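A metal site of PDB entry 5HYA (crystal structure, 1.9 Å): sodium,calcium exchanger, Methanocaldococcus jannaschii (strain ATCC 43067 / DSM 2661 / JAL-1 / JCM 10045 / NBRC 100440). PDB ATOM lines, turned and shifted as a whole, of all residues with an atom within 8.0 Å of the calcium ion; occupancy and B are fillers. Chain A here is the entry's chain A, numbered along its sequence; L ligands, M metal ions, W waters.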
ATOM      1  N   ALA A 115      21.598  21.597   7.938  1.00  0.00           N
ATOM      2  CA  ALA A 115      22.446  22.746   8.264  1.00  0.00           C
ATOM      3  C   ALA A 115      23.490  22.410   9.334  1.00  0.00           C
ATOM      4  O   ALA A 115      24.664  22.774   9.209  1.00  0.00           O
ATOM      5  CB  ALA A 115      21.593  23.930   8.731  1.00  0.00           C
ATOM      6  N   ALA A 116      23.059  21.718  10.387  1.00  0.00           N
ATOM      7  CA  ALA A 116      23.964  21.388  11.484  1.00  0.00           C
ATOM      8  C   ALA A 116      25.122  20.519  10.985  1.00  0.00           C
ATOM      9  O   ALA A 116      26.281  20.754  11.334  1.00  0.00           O
ATOM     10  CB  ALA A 116      23.217  20.666  12.611  1.00  0.00           C
ATOM     11  N   VAL A 117      24.796  19.559  10.138  1.00  0.00           N
ATOM     12  CA  VAL A 117      25.798  18.621   9.624  1.00  0.00           C
ATOM     13  C   VAL A 117      26.819  19.320   8.716  1.00  0.00           C
ATOM     14  O   VAL A 117      28.028  19.218   8.928  1.00  0.00           O
ATOM     15  CB  VAL A 117      25.132  17.452   8.870  1.00  0.00           C
ATOM     16  CG1 VAL A 117      26.153  16.665   8.051  1.00  0.00           C
ATOM     17  CG2 VAL A 117      24.419  16.534   9.868  1.00  0.00           C
ATOM     18  N   ILE A 118      26.344  20.034   7.702  1.00  0.00           N
ATOM     19  CA  ILE A 118      27.291  20.702   6.808  1.00  0.00           C
ATOM     20  C   ILE A 118      28.020  21.839   7.535  1.00  0.00           C
ATOM     21  O   ILE A 118      29.065  22.294   7.078  1.00  0.00           O
ATOM     22  CB  ILE A 118      26.636  21.255   5.521  1.00  0.00           C
ATOM     23  CG1 ILE A 118      25.790  22.506   5.812  1.00  0.00           C
ATOM     24  CG2 ILE A 118      25.862  20.156   4.790  1.00  0.00           C
ATOM     25  CD1 ILE A 118      25.172  23.108   4.566  1.00  0.00           C
ATOM     26  N   GLY A 119      27.494  22.268   8.670  1.00  0.00           N
ATOM     27  CA  GLY A 119      28.135  23.321   9.434  1.00  0.00           C
ATOM     28  C   GLY A 119      29.185  22.872  10.454  1.00  0.00           C
ATOM     29  O   GLY A 119      29.772  23.712  11.129  1.00  0.00           O
ATOM     30  N   ILE A 120      29.418  21.572  10.562  1.00  0.00           N
ATOM     31  CA  ILE A 120      30.347  21.046  11.573  1.00  0.00           C
ATOM     32  C   ILE A 120      31.752  21.629  11.403  1.00  0.00           C
ATOM     33  O   ILE A 120      32.452  21.897  12.381  1.00  0.00           O
ATOM     34  CB  ILE A 120      30.410  19.494  11.529  1.00  0.00           C
ATOM     35  CG1 ILE A 120      29.107  18.899  12.067  1.00  0.00           C
ATOM     36  CG2 ILE A 120      31.561  18.961  12.384  1.00  0.00           C
ATOM     37  CD1 ILE A 120      28.941  17.424  11.750  1.00  0.00           C
ATOM     38  N   ASP A 121      32.144  21.869  10.155  1.00  0.00           N
ATOM     39  CA  ASP A 121      33.440  22.492   9.881  1.00  0.00           C
ATOM     40  C   ASP A 121      33.264  23.962   9.520  1.00  0.00           C
ATOM     41  O   ASP A 121      34.098  24.532   8.822  1.00  0.00           O
ATOM     42  CB  ASP A 121      34.178  21.723   8.771  1.00  0.00           C
ATOM     43  CG  ASP A 121      33.396  21.686   7.467  1.00  0.00           C
ATOM     44  OD1 ASP A 121      32.191  22.028   7.447  1.00  0.00           O
ATOM     45  OD2 ASP A 121      33.995  21.296   6.443  1.00  0.00           O
ATOM     46  N   GLY A 122      32.195  24.570  10.009  1.00  0.00           N
ATOM     47  CA  GLY A 122      31.864  25.934   9.655  1.00  0.00           C
ATOM     48  C   GLY A 122      31.077  26.006   8.350  1.00  0.00           C
ATOM     49  O   GLY A 122      30.824  24.994   7.713  1.00  0.00           O
ATOM     50  N   PHE A 123      30.683  27.212   7.952  1.00  0.00           N
ATOM     51  CA  PHE A 123      29.879  27.368   6.757  1.00  0.00           C
ATOM     52  C   PHE A 123      30.646  28.126   5.685  1.00  0.00           C
ATOM     53  O   PHE A 123      31.059  29.277   5.899  1.00  0.00           O
ATOM     54  CB  PHE A 123      28.576  28.102   7.095  1.00  0.00           C
ATOM     55  CG  PHE A 123      27.647  27.317   7.983  1.00  0.00           C
ATOM     56  CD1 PHE A 123      26.703  26.476   7.443  1.00  0.00           C
ATOM     57  CD2 PHE A 123      27.719  27.455   9.361  1.00  0.00           C
ATOM     58  CE1 PHE A 123      25.834  25.764   8.253  1.00  0.00           C
ATOM     59  CE2 PHE A 123      26.852  26.737  10.183  1.00  0.00           C
ATOM     60  CZ  PHE A 123      25.918  25.896   9.633  1.00  0.00           C
ATOM     61  N   SER A 124      30.831  27.488   4.539  1.00  0.00           N
ATOM     62  CA  SER A 124      31.491  28.124   3.409  1.00  0.00           C
ATOM     63  C   SER A 124      30.457  28.778   2.529  1.00  0.00           C
ATOM     64  O   SER A 124      29.252  28.633   2.745  1.00  0.00           O
ATOM     65  CB  SER A 124      32.292  27.116   2.583  1.00  0.00           C
ATOM     66  OG  SER A 124      31.392  26.236   1.912  1.00  0.00           O
ATOM     67  N   TRP A 125      30.926  29.483   1.508  1.00  0.00           N
ATOM     68  CA  TRP A 125      30.026  30.177   0.608  1.00  0.00           C
ATOM     69  C   TRP A 125      29.202  29.162  -0.184  1.00  0.00           C
ATOM     70  O   TRP A 125      28.073  29.457  -0.571  1.00  0.00           O
ATOM     71  CB  TRP A 125      30.810  31.107  -0.325  1.00  0.00           C
ATOM     72  CG  TRP A 125      31.752  30.393  -1.245  1.00  0.00           C
ATOM     73  CD1 TRP A 125      33.065  30.081  -1.005  1.00  0.00           C
ATOM     74  CD2 TRP A 125      31.447  29.887  -2.557  1.00  0.00           C
ATOM     75  NE1 TRP A 125      33.595  29.426  -2.094  1.00  0.00           N
ATOM     76  CE2 TRP A 125      32.618  29.289  -3.051  1.00  0.00           C
ATOM     77  CE3 TRP A 125      30.295  29.897  -3.354  1.00  0.00           C
ATOM     78  CZ2 TRP A 125      32.679  28.703  -4.317  1.00  0.00           C
ATOM     79  CZ3 TRP A 125      30.364  29.316  -4.611  1.00  0.00           C
ATOM     80  CH2 TRP A 125      31.545  28.721  -5.073  1.00  0.00           C
ATOM     81  N   ILE A 126      29.743  27.972  -0.405  1.00  0.00           N
ATOM     82  CA  ILE A 126      28.996  26.918  -1.095  1.00  0.00           C
ATOM     83  C   ILE A 126      27.897  26.356  -0.194  1.00  0.00           C
ATOM     84  O   ILE A 126      26.799  26.061  -0.656  1.00  0.00           O
ATOM     85  CB  ILE A 126      29.894  25.759  -1.565  1.00  0.00           C
ATOM     86  CG1 ILE A 126      31.012  26.267  -2.449  1.00  0.00           C
ATOM     87  CG2 ILE A 126      29.079  24.748  -2.357  1.00  0.00           C
ATOM     88  CD1 ILE A 126      31.958  25.182  -2.915  1.00  0.00           C
ATOM     89  N   ASP A 127      28.184  26.232   1.102  1.00  0.00           N
ATOM     90  CA  ASP A 127      27.148  25.889   2.071  1.00  0.00           C
ATOM     91  C   ASP A 127      26.002  26.895   1.988  1.00  0.00           C
ATOM     92  O   ASP A 127      24.829  26.523   1.981  1.00  0.00           O
ATOM     93  CB  ASP A 127      27.707  25.838   3.506  1.00  0.00           C
ATOM     94  CG  ASP A 127      28.699  24.699   3.718  1.00  0.00           C
ATOM     95  OD1 ASP A 127      28.566  23.646   3.063  1.00  0.00           O
ATOM     96  OD2 ASP A 127      29.610  24.873   4.555  1.00  0.00           O
ATOM     97  N   GLY A 128      26.355  28.183   1.937  1.00  0.00           N
ATOM     98  CA  GLY A 128      25.369  29.243   1.852  1.00  0.00           C
ATOM     99  C   GLY A 128      24.494  29.142   0.622  1.00  0.00           C
ATOM    100  O   GLY A 128      23.269  29.298   0.696  1.00  0.00           O
ATOM    101  N   HIS A 253      34.050  32.856   5.342  1.00  0.00           N
ATOM    102  CA  HIS A 253      33.744  31.569   5.962  1.00  0.00           C
ATOM    103  C   HIS A 253      33.244  31.805   7.396  1.00  0.00           C
ATOM    104  O   HIS A 253      33.826  32.598   8.137  1.00  0.00           O
ATOM    105  CB  HIS A 253      34.981  30.667   5.960  1.00  0.00           C
ATOM    106  CG  HIS A 253      34.710  29.273   6.416  1.00  0.00           C
ATOM    107  ND1 HIS A 253      34.269  28.281   5.526  1.00  0.00           N
ATOM    108  CD2 HIS A 253      34.788  28.676   7.601  1.00  0.00           C
ATOM    109  CE1 HIS A 253      34.106  27.165   6.182  1.00  0.00           C
ATOM    110  NE2 HIS A 253      34.404  27.349   7.462  1.00  0.00           N
ATOM    111  N   LEU A 254      32.149  31.154   7.780  1.00  0.00           N
ATOM    112  CA  LEU A 254      31.617  31.328   9.125  1.00  0.00           C
ATOM    113  C   LEU A 254      32.134  30.207  10.000  1.00  0.00           C
ATOM    114  O   LEU A 254      32.103  29.047   9.625  1.00  0.00           O
ATOM    115  CB  LEU A 254      30.085  31.328   9.112  1.00  0.00           C
ATOM    116  CG  LEU A 254      29.397  32.296   8.151  1.00  0.00           C
ATOM    117  CD1 LEU A 254      27.867  32.202   8.292  1.00  0.00           C
ATOM    118  CD2 LEU A 254      29.902  33.733   8.331  1.00  0.00           C
ATOM    119  N   ALA A 256      32.411  27.367  12.893  1.00  0.00           N
ATOM    120  CA  ALA A 256      31.410  26.441  13.419  1.00  0.00           C
ATOM    121  C   ALA A 256      30.903  26.883  14.781  1.00  0.00           C
ATOM    122  O   ALA A 256      31.633  27.430  15.596  1.00  0.00           O
ATOM    123  CB  ALA A 256      31.984  25.040  13.503  1.00  0.00           C
HETATM  124  C1  LIG L   1      14.061  15.776   0.020  1.00  0.00           C
HETATM  125  C2  LIG L   1      19.116  15.869   6.093  1.00  0.00           C
HETATM  126  C3  LIG L   1      19.985  15.431   7.303  1.00  0.00           C
HETATM  127  C4  LIG L   1      13.496  14.860   1.073  1.00  0.00           C
HETATM  128  C5  LIG L   1      19.068  14.831   4.949  1.00  0.00           C
HETATM  129  C6  LIG L   1      21.010  14.303   6.930  1.00  0.00           C
HETATM  130  C7  LIG L   1      30.067  20.707   4.484  1.00  0.00           C
HETATM  131  C8  LIG L   1      14.148  13.470   0.972  1.00  0.00           C
HETATM  132  C9  LIG L   1      17.606  14.550   4.471  1.00  0.00           C
HETATM  133  C10 LIG L   1      22.454  14.864   6.686  1.00  0.00           C
HETATM  134  C11 LIG L   1      15.675  13.522   1.220  1.00  0.00           C
HETATM  135  C12 LIG L   1      17.482  14.036   3.010  1.00  0.00           C
HETATM  136  C13 LIG L   1      22.753  15.151   5.166  1.00  0.00           C
HETATM  137  C14 LIG L   1      15.970  13.935   2.663  1.00  0.00           C
HETATM  138  C15 LIG L   1      24.156  14.712   4.709  1.00  0.00           C
HETATM  139  C16 LIG L   1      24.960  15.836   4.014  1.00  0.00           C
HETATM  140  C17 LIG L   1      26.456  15.862   4.455  1.00  0.00           C
HETATM  141  C18 LIG L   1      27.409  16.413   3.365  1.00  0.00           C
HETATM  142  C19 LIG L   1      30.670  18.337   4.174  1.00  0.00           C
HETATM  143  C20 LIG L   1      28.776  16.820   3.924  1.00  0.00           C
HETATM  144  C21 LIG L   1      31.052  19.750   3.827  1.00  0.00           C
HETATM  145  O1  LIG L   1      29.302  16.105   4.744  1.00  0.00           O
HETATM  146  O2  LIG L   1      30.403  22.034   4.095  1.00  0.00           O
HETATM  147  O3  LIG L   1      32.347  20.055   4.283  1.00  0.00           O
HETATM  148  O4  LIG L   1      29.420  18.020   3.495  1.00  0.00           O
HETATM  149 CA    CA M   1      30.801  23.401   6.022  1.00  0.00          CA
HETATM  150  O   HOH W   1      32.892  24.404   5.154  1.00  0.00           O
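The calcium ion is bound by O of Ile 118 (2.3 Å), O of Gly 122 (2.3 Å), OD2 of Asp 127 (2.4 Å), O2 of the ligand (2.4 Å), OD1 of Asp 121 (2.4 Å) and water W1 (2.5 Å).
The calcium ion has six donor atoms within binding distance.
Four residues have an atom within 4 Å of the calcium ion: Ile 118, Asp 121, Gly 122 and Asp 127.
N of Asp 127 lies within hydrogen-bond range of OG of Ser 124 (3.3 Å).
A ring nitrogen (NE2) of His 253 is in hydrogen-bond range of the backbone carbonyl oxygen of Asp 121 (3.1 Å).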
